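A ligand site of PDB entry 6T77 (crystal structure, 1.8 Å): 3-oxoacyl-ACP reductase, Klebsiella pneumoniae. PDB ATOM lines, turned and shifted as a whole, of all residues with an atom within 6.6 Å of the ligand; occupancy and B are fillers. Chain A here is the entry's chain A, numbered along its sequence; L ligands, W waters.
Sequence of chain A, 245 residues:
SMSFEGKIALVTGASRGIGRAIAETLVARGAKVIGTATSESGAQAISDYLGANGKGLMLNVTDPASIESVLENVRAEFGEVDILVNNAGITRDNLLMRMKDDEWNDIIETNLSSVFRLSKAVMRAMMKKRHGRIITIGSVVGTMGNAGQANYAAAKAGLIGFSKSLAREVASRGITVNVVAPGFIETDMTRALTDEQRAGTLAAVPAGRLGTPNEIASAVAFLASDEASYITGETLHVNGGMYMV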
ATOM      1  N   THR A  12      -2.749 -10.785  20.785  1.00  0.00           N
ATOM      2  CA  THR A  12      -2.239 -11.614  19.718  1.00  0.00           C
ATOM      3  C   THR A  12      -1.218 -12.601  20.304  1.00  0.00           C
ATOM      4  O   THR A  12      -0.448 -12.249  21.155  1.00  0.00           O
ATOM      5  CB  THR A  12      -1.626 -10.776  18.589  1.00  0.00           C
ATOM      6  OG1 THR A  12      -0.443 -10.102  19.064  1.00  0.00           O
ATOM      7  CG2 THR A  12      -2.626  -9.790  18.079  1.00  0.00           C
ATOM      8  N   GLY A  13      -1.194 -13.816  19.799  1.00  0.00           N
ATOM      9  CA  GLY A  13      -0.261 -14.829  20.281  1.00  0.00           C
ATOM     10  C   GLY A  13      -0.518 -15.255  21.744  1.00  0.00           C
ATOM     11  O   GLY A  13       0.376 -15.149  22.601  1.00  0.00           O
ATOM     12  N   ALA A  14      -1.724 -15.710  22.015  1.00  0.00           N
ATOM     13  CA  ALA A  14      -2.162 -15.958  23.369  1.00  0.00           C
ATOM     14  C   ALA A  14      -2.192 -17.438  23.780  1.00  0.00           C
ATOM     15  O   ALA A  14      -2.799 -17.798  24.796  1.00  0.00           O
ATOM     16  CB  ALA A  14      -3.509 -15.284  23.622  1.00  0.00           C
ATOM     17  N   SER A  15      -1.512 -18.281  23.014  1.00  0.00           N
ATOM     18  CA  SER A  15      -1.597 -19.754  23.233  1.00  0.00           C
ATOM     19  C   SER A  15      -1.008 -20.170  24.580  1.00  0.00           C
ATOM     20  O   SER A  15      -1.528 -21.082  25.257  1.00  0.00           O
ATOM     21  CB  SER A  15      -0.804 -20.447  22.154  1.00  0.00           C
ATOM     22  OG  SER A  15      -1.486 -20.314  20.961  1.00  0.00           O
ATOM     23  N   ARG A  16       0.083 -19.552  24.944  1.00  0.00           N
ATOM     24  CA  ARG A  16       0.895 -19.987  26.077  1.00  0.00           C
ATOM     25  C   ARG A  16       1.750 -18.843  26.593  1.00  0.00           C
ATOM     26  O   ARG A  16       1.693 -17.752  26.091  1.00  0.00           O
ATOM     27  CB  ARG A  16       1.752 -21.192  25.662  1.00  0.00           C
ATOM     28  CG  ARG A  16       2.848 -20.883  24.694  1.00  0.00           C
ATOM     29  CD  ARG A  16       3.451 -22.166  24.110  1.00  0.00           C
ATOM     30  NE  ARG A  16       2.647 -22.666  23.002  1.00  0.00           N
ATOM     31  CZ  ARG A  16       2.638 -22.155  21.746  1.00  0.00           C
ATOM     32  NH1 ARG A  16       3.392 -21.103  21.410  1.00  0.00           N
ATOM     33  NH2 ARG A  16       1.841 -22.708  20.821  1.00  0.00           N
ATOM     34  N   GLY A  17       2.558 -19.148  27.638  1.00  0.00           N
ATOM     35  CA  GLY A  17       3.544 -18.256  28.151  1.00  0.00           C
ATOM     36  C   GLY A  17       2.983 -16.878  28.454  1.00  0.00           C
ATOM     37  O   GLY A  17       1.949 -16.727  29.102  1.00  0.00           O
ATOM     38  N   ILE A  18       3.701 -15.860  27.973  1.00  0.00           N
ATOM     39  CA  ILE A  18       3.373 -14.498  28.266  1.00  0.00           C
ATOM     40  C   ILE A  18       1.992 -14.118  27.731  1.00  0.00           C
ATOM     41  O   ILE A  18       1.176 -13.478  28.426  1.00  0.00           O
ATOM     42  CB  ILE A  18       4.476 -13.558  27.703  1.00  0.00           C
ATOM     43  CG1 ILE A  18       5.747 -13.719  28.525  1.00  0.00           C
ATOM     44  CG2 ILE A  18       4.006 -12.111  27.625  1.00  0.00           C
ATOM     45  CD1 ILE A  18       7.013 -13.135  27.881  1.00  0.00           C
ATOM     46  N   GLY A  19       1.698 -14.467  26.487  1.00  0.00           N
ATOM     47  CA  GLY A  19       0.391 -14.058  25.909  1.00  0.00           C
ATOM     48  C   GLY A  19      -0.818 -14.680  26.667  1.00  0.00           C
ATOM     49  O   GLY A  19      -1.812 -14.002  26.920  1.00  0.00           O
ATOM     50  N   THR A  36      -5.436 -14.859  20.224  1.00  0.00           N
ATOM     51  CA  THR A  36      -5.206 -15.464  18.932  1.00  0.00           C
ATOM     52  C   THR A  36      -4.043 -16.457  18.885  1.00  0.00           C
ATOM     53  O   THR A  36      -3.089 -16.383  19.658  1.00  0.00           O
ATOM     54  CB  THR A  36      -5.026 -14.393  17.825  1.00  0.00           C
ATOM     55  OG1 THR A  36      -3.699 -13.838  17.884  1.00  0.00           O
ATOM     56  CG2 THR A  36      -6.040 -13.228  17.987  1.00  0.00           C
ATOM     57  N   ALA A  37      -4.180 -17.356  17.919  1.00  0.00           N
ATOM     58  CA  ALA A  37      -3.161 -18.343  17.549  1.00  0.00           C
ATOM     59  C   ALA A  37      -3.135 -18.474  16.036  1.00  0.00           C
ATOM     60  O   ALA A  37      -3.997 -17.955  15.393  1.00  0.00           O
ATOM     61  CB  ALA A  37      -3.511 -19.690  18.148  1.00  0.00           C
ATOM     62  N   THR A  38      -2.133 -19.145  15.491  1.00  0.00           N
ATOM     63  CA  THR A  38      -1.993 -19.251  14.021  1.00  0.00           C
ATOM     64  C   THR A  38      -2.704 -20.444  13.405  1.00  0.00           C
ATOM     65  O   THR A  38      -2.728 -20.564  12.208  1.00  0.00           O
ATOM     66  CB  THR A  38      -0.498 -19.328  13.622  1.00  0.00           C
ATOM     67  OG1 THR A  38       0.052 -20.495  14.225  1.00  0.00           O
ATOM     68  CG2 THR A  38       0.275 -18.136  14.114  1.00  0.00           C
ATOM     69  N   SER A  39      -3.306 -21.319  14.197  1.00  0.00           N
ATOM     70  CA  SER A  39      -4.078 -22.487  13.701  1.00  0.00           C
ATOM     71  C   SER A  39      -5.439 -22.536  14.369  1.00  0.00           C
ATOM     72  O   SER A  39      -5.653 -21.958  15.442  1.00  0.00           O
ATOM     73  CB  SER A  39      -3.339 -23.769  14.051  1.00  0.00           C
ATOM     74  OG  SER A  39      -3.235 -23.901  15.467  1.00  0.00           O
ATOM     75  N   GLY A  42      -5.069 -24.296  17.803  1.00  0.00           N
ATOM     76  CA  GLY A  42      -4.541 -23.317  18.757  1.00  0.00           C
ATOM     77  C   GLY A  42      -5.613 -22.327  19.247  1.00  0.00           C
ATOM     78  O   GLY A  42      -5.695 -22.014  20.390  1.00  0.00           O
ATOM     79  N   ILE A  46      -7.306 -21.784  23.098  1.00  0.00           N
ATOM     80  CA  ILE A  46      -7.541 -20.479  23.718  1.00  0.00           C
ATOM     81  C   ILE A  46      -9.005 -20.336  24.173  1.00  0.00           C
ATOM     82  O   ILE A  46      -9.277 -19.886  25.290  1.00  0.00           O
ATOM     83  CB  ILE A  46      -7.080 -19.302  22.824  1.00  0.00           C
ATOM     84  CG1 ILE A  46      -5.582 -19.287  22.697  1.00  0.00           C
ATOM     85  CG2 ILE A  46      -7.522 -17.951  23.395  1.00  0.00           C
ATOM     86  CD1 ILE A  46      -5.005 -18.485  21.566  1.00  0.00           C
ATOM     87  N   LEU A  59      -5.428 -16.059  13.774  1.00  0.00           N
ATOM     88  CA  LEU A  59      -4.913 -14.835  13.188  1.00  0.00           C
ATOM     89  C   LEU A  59      -3.507 -15.044  12.697  1.00  0.00           C
ATOM     90  O   LEU A  59      -2.676 -15.583  13.420  1.00  0.00           O
ATOM     91  CB  LEU A  59      -4.914 -13.726  14.222  1.00  0.00           C
ATOM     92  CG  LEU A  59      -4.297 -12.389  13.841  1.00  0.00           C
ATOM     93  CD1 LEU A  59      -5.058 -11.719  12.763  1.00  0.00           C
ATOM     94  CD2 LEU A  59      -4.255 -11.488  15.061  1.00  0.00           C
ATOM     95  N   ASN A  60      -3.245 -14.577  11.497  1.00  0.00           N
ATOM     96  CA  ASN A  60      -1.903 -14.395  10.988  1.00  0.00           C
ATOM     97  C   ASN A  60      -1.665 -12.859  10.903  1.00  0.00           C
ATOM     98  O   ASN A  60      -2.304 -12.176  10.081  1.00  0.00           O
ATOM     99  CB  ASN A  60      -1.757 -15.075   9.650  1.00  0.00           C
ATOM    100  CG  ASN A  60      -0.382 -14.892   9.052  1.00  0.00           C
ATOM    101  OD1 ASN A  60       0.499 -14.215   9.598  1.00  0.00           O
ATOM    102  ND2 ASN A  60      -0.174 -15.502   7.906  1.00  0.00           N
ATOM    103  N   VAL A  61      -0.790 -12.347  11.766  1.00  0.00           N
ATOM    104  CA  VAL A  61      -0.585 -10.917  11.847  1.00  0.00           C
ATOM    105  C   VAL A  61       0.183 -10.348  10.638  1.00  0.00           C
ATOM    106  O   VAL A  61       0.314  -9.130  10.517  1.00  0.00           O
ATOM    107  CB  VAL A  61       0.117 -10.438  13.140  1.00  0.00           C
ATOM    108  CG1 VAL A  61      -0.657 -10.796  14.373  1.00  0.00           C
ATOM    109  CG2 VAL A  61       1.530 -10.972  13.235  1.00  0.00           C
ATOM    110  N   THR A  62       0.674 -11.224   9.737  1.00  0.00           N
ATOM    111  CA  THR A  62       1.297 -10.743   8.495  1.00  0.00           C
ATOM    112  C   THR A  62       0.334 -10.656   7.335  1.00  0.00           C
ATOM    113  O   THR A  62       0.686 -10.171   6.259  1.00  0.00           O
ATOM    114  CB  THR A  62       2.503 -11.595   8.093  1.00  0.00           C
ATOM    115  OG1 THR A  62       2.062 -12.884   7.643  1.00  0.00           O
ATOM    116  CG2 THR A  62       3.487 -11.695   9.259  1.00  0.00           C
ATOM    117  N   ASN A  87       1.465  -9.219  21.193  1.00  0.00           N
ATOM    118  CA  ASN A  87       2.393 -10.258  21.775  1.00  0.00           C
ATOM    119  C   ASN A  87       2.961 -11.210  20.746  1.00  0.00           C
ATOM    120  O   ASN A  87       4.010 -11.810  20.969  1.00  0.00           O
ATOM    121  CB  ASN A  87       1.757 -11.006  22.944  1.00  0.00           C
ATOM    122  CG  ASN A  87       2.681 -12.034  23.547  1.00  0.00           C
ATOM    123  OD1 ASN A  87       3.639 -11.695  24.187  1.00  0.00           O
ATOM    124  ND2 ASN A  87       2.405 -13.314  23.278  1.00  0.00           N
ATOM    125  N   ALA A  88       2.325 -11.325  19.615  1.00  0.00           N
ATOM    126  CA  ALA A  88       2.753 -12.260  18.567  1.00  0.00           C
ATOM    127  C   ALA A  88       4.155 -11.955  18.116  1.00  0.00           C
ATOM    128  O   ALA A  88       4.499 -10.809  17.913  1.00  0.00           O
ATOM    129  CB  ALA A  88       1.813 -12.172  17.365  1.00  0.00           C
ATOM    130  N   GLY A  89       4.997 -12.974  17.984  1.00  0.00           N
ATOM    131  CA  GLY A  89       6.362 -12.744  17.543  1.00  0.00           C
ATOM    132  C   GLY A  89       7.078 -14.052  17.362  1.00  0.00           C
ATOM    133  O   GLY A  89       6.624 -15.095  17.859  1.00  0.00           O
ATOM    134  N   ILE A  90       8.127 -14.029  16.563  1.00  0.00           N
ATOM    135  CA  ILE A  90       8.922 -15.224  16.277  1.00  0.00           C
ATOM    136  C   ILE A  90      10.422 -14.888  16.342  1.00  0.00           C
ATOM    137  O   ILE A  90      10.800 -13.699  16.289  1.00  0.00           O
ATOM    138  CB  ILE A  90       8.605 -15.763  14.869  1.00  0.00           C
ATOM    139  CG1 ILE A  90       8.857 -14.709  13.768  1.00  0.00           C
ATOM    140  CG2 ILE A  90       7.179 -16.358  14.803  1.00  0.00           C
ATOM    141  CD1 ILE A  90       8.747 -15.201  12.329  1.00  0.00           C
ATOM    142  N   THR A 110       6.841 -10.085  10.810  1.00  0.00           N
ATOM    143  CA  THR A 110       6.072 -10.667  11.884  1.00  0.00           C
ATOM    144  C   THR A 110       6.163  -9.875  13.156  1.00  0.00           C
ATOM    145  O   THR A 110       5.132  -9.733  13.824  1.00  0.00           O
ATOM    146  CB  THR A 110       6.469 -12.145  12.148  1.00  0.00           C
ATOM    147  OG1 THR A 110       6.400 -12.883  10.907  1.00  0.00           O
ATOM    148  CG2 THR A 110       5.573 -12.760  13.172  1.00  0.00           C
ATOM    149  N   THR A 187       9.567 -19.914  30.176  1.00  0.00           N
ATOM    150  CA  THR A 187       8.684 -20.212  29.025  1.00  0.00           C
ATOM    151  C   THR A 187       9.196 -21.492  28.391  1.00  0.00           C
ATOM    152  O   THR A 187      10.278 -22.021  28.800  1.00  0.00           O
ATOM    153  CB  THR A 187       8.717 -19.162  27.861  1.00  0.00           C
ATOM    154  OG1 THR A 187      10.055 -19.094  27.311  1.00  0.00           O
ATOM    155  CG2 THR A 187       8.267 -17.761  28.327  1.00  0.00           C
ATOM    156  N   ASP A 188       8.460 -22.035  27.412  1.00  0.00           N
ATOM    157  CA  ASP A 188       8.935 -23.224  26.672  1.00  0.00           C
ATOM    158  C   ASP A 188      10.354 -23.023  26.140  1.00  0.00           C
ATOM    159  O   ASP A 188      11.193 -23.895  26.305  1.00  0.00           O
ATOM    160  CB  ASP A 188       8.003 -23.552  25.480  1.00  0.00           C
ATOM    161  CG  ASP A 188       6.655 -24.080  25.919  1.00  0.00           C
ATOM    162  OD1 ASP A 188       6.471 -24.390  27.085  1.00  0.00           O
ATOM    163  OD2 ASP A 188       5.746 -24.177  25.064  1.00  0.00           O
ATOM    164  N   MET A 189      10.599 -21.852  25.537  1.00  0.00           N
ATOM    165  CA  MET A 189      11.932 -21.432  25.065  1.00  0.00           C
ATOM    166  C   MET A 189      13.050 -21.682  26.109  1.00  0.00           C
ATOM    167  O   MET A 189      14.010 -22.415  25.847  1.00  0.00           O
ATOM    168  CB  MET A 189      11.913 -19.938  24.683  1.00  0.00           C
ATOM    169  CG  MET A 189      13.175 -19.392  24.026  1.00  0.00           C
ATOM    170  SD  MET A 189      13.161 -17.569  23.890  1.00  0.00           S
ATOM    171  CE  MET A 189      13.753 -17.069  25.509  1.00  0.00           C
HETATM  172  P1  LIG L   1       5.948 -17.837  22.072  1.00  0.00           P
HETATM  173  O1  LIG L   1       6.696 -16.733  23.044  1.00  0.00           O
HETATM  174  O2  LIG L   1       4.951 -18.751  22.789  1.00  0.00           O
HETATM  175  O3  LIG L   1       5.084 -16.713  21.280  1.00  0.00           O
HETATM  176  C1  LIG L   1       4.717 -16.849  19.927  1.00  0.00           C
HETATM  177  C2  LIG L   1       3.247 -16.506  19.798  1.00  0.00           C
HETATM  178  O4  LIG L   1       3.108 -15.615  18.674  1.00  0.00           O
HETATM  179  C3  LIG L   1       2.440 -17.774  19.550  1.00  0.00           C
HETATM  180  O5  LIG L   1       1.148 -17.667  20.189  1.00  0.00           O
HETATM  181  C4  LIG L   1       2.339 -17.803  18.055  1.00  0.00           C
HETATM  182  O6  LIG L   1       1.185 -18.508  17.649  1.00  0.00           O
HETATM  183  C5  LIG L   1       2.240 -16.307  17.746  1.00  0.00           C
HETATM  184  N1  LIG L   1       2.650 -16.077  16.353  1.00  0.00           N
HETATM  185  C6  LIG L   1       3.788 -16.471  15.701  1.00  0.00           C
HETATM  186  N2  LIG L   1       3.739 -16.087  14.398  1.00  0.00           N
HETATM  187  C7  LIG L   1       2.553 -15.486  14.212  1.00  0.00           C
HETATM  188  C8  LIG L   1       1.851 -14.887  13.063  1.00  0.00           C
HETATM  189  N3  LIG L   1       2.447 -14.841  11.864  1.00  0.00           N
HETATM  190  N4  LIG L   1       0.643 -14.338  13.306  1.00  0.00           N
HETATM  191  C9  LIG L   1       0.053 -14.386  14.513  1.00  0.00           C
HETATM  192  N5  LIG L   1       0.613 -14.944  15.614  1.00  0.00           N
HETATM  193  C10 LIG L   1       1.839 -15.483  15.493  1.00  0.00           C
HETATM  194  O7  LIG L   1       7.015 -18.430  21.169  1.00  0.00           O
HETATM  195  P2  LIG L   1       1.058 -20.083  17.794  1.00  0.00           P
HETATM  196  O8  LIG L   1       2.458 -20.584  17.702  1.00  0.00           O
HETATM  197  O9  LIG L   1       0.543 -20.266  19.205  1.00  0.00           O
HETATM  198  O10 LIG L   1       0.055 -20.483  16.808  1.00  0.00           O
HETATM  199  O   HOH W   1       5.878 -19.150  25.384  1.00  0.00           O
HETATM  200  O   HOH W   2       6.349 -18.839  17.597  1.00  0.00           O
HETATM  201  O   HOH W   3       5.170 -15.174  10.683  1.00  0.00           O
HETATM  202  O   HOH W   4       5.840 -16.428  25.876  1.00  0.00           O
HETATM  203  O   HOH W   5      -2.170 -15.404  16.299  1.00  0.00           O
HETATM  204  O   HOH W   6      -1.647 -22.660  16.916  1.00  0.00           O
HETATM  205  O   HOH W   7       1.975 -17.779  23.091  1.00  0.00           O
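O2 of the ligand lies within salt-bridge range of NH1 of Arg 16. O4 of the ligand lies within hydrogen-bond range of N of Gly 89 (3.3 Å). N4 of the ligand is in hydrogen-bond range of N of Val 61. The side-chain amide oxygen (OD1) of Asn 60 lies within hydrogen-bond range of a nitrogen (N3) of the ligand, 3.1 Å away. O10 of the ligand lies within hydrogen-bond range of OG1 of Thr 38 (2.6 Å). The side-chain hydroxyl (OG) of Ser 15 is in hydrogen-bond range of an oxygen (O9) of the ligand, at 2.7 Å. The backbone NH (N) of Thr 38 lies within hydrogen-bond range of an oxygen (O10) of the ligand, 2.9 Å away.
The side-chain amide oxygen of Asn 60 sits at hydrogen-bond distance from the side-chain hydroxyl of Thr 62 (2.8 Å). N of Gly 13 lies within hydrogen-bond range of OG1 of Thr 36 (3.2 Å). The backbone carbonyl oxygen (O) of Thr 36 is in hydrogen-bond range of the backbone NH (N) of Ala 14, 2.8 Å away. The backbone carbonyl oxygen (O) of Ala 37 is in hydrogen-bond range of the backbone NH (N) of Leu 59. OG1 of Thr 12 sits at hydrogen-bond distance from N of Ala 88 (3.1 Å). O of Gly 13 lies within hydrogen-bond range of ND2 of Asn 87.
Gly 13 touches the ligand. Ala 14 touches the ligand (N to O5, 3.9 Å). Ala 37 touches the ligand (C to O10, 3.8 Å). Leu 59 touches the ligand (O to C9, 3.2 Å). Ala 88 touches the ligand. CG2 of Ile 90 touches N2 of the ligand (3.5 Å). Thr 110 touches the ligand (CG2 to N3, 3.98 Å). Hydrophobic or aromatic side chains that line the ligand: Ala 37, Val 61, Ala 88 and Ile 90. 13 residues have an atom within 4 Å of the ligand: Gly 13, Ala 14, Ser 15, Arg 16, Ala 37, Thr 38, Leu 59, Asn 60, Val 61, Ala 88, Gly 89, Ile 90 and Thr 110.
Water W6 bridges OG of Ser 39 (2.5 Å) and O10 of the ligand (2.8 Å). Water W5 lies within hydrogen-bond range of the side-chain hydroxyl of Thr 36, a nitrogen (N5) of the ligand, the backbone carbonyl oxygen of Leu 59 and the backbone NH of Ala 37. Water W4 lies within hydrogen-bond range of an oxygen (O1) of the ligand and the backbone NH (N) of Ile 18. Water W3 lies within hydrogen-bond range of the side-chain hydroxyl of Thr 110 (2.6 Å) and a nitrogen (N3) of the ligand (3.0 Å). Water W7 lies within hydrogen-bond range of O of Arg 16, O5 of the ligand and O of Gly 13.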
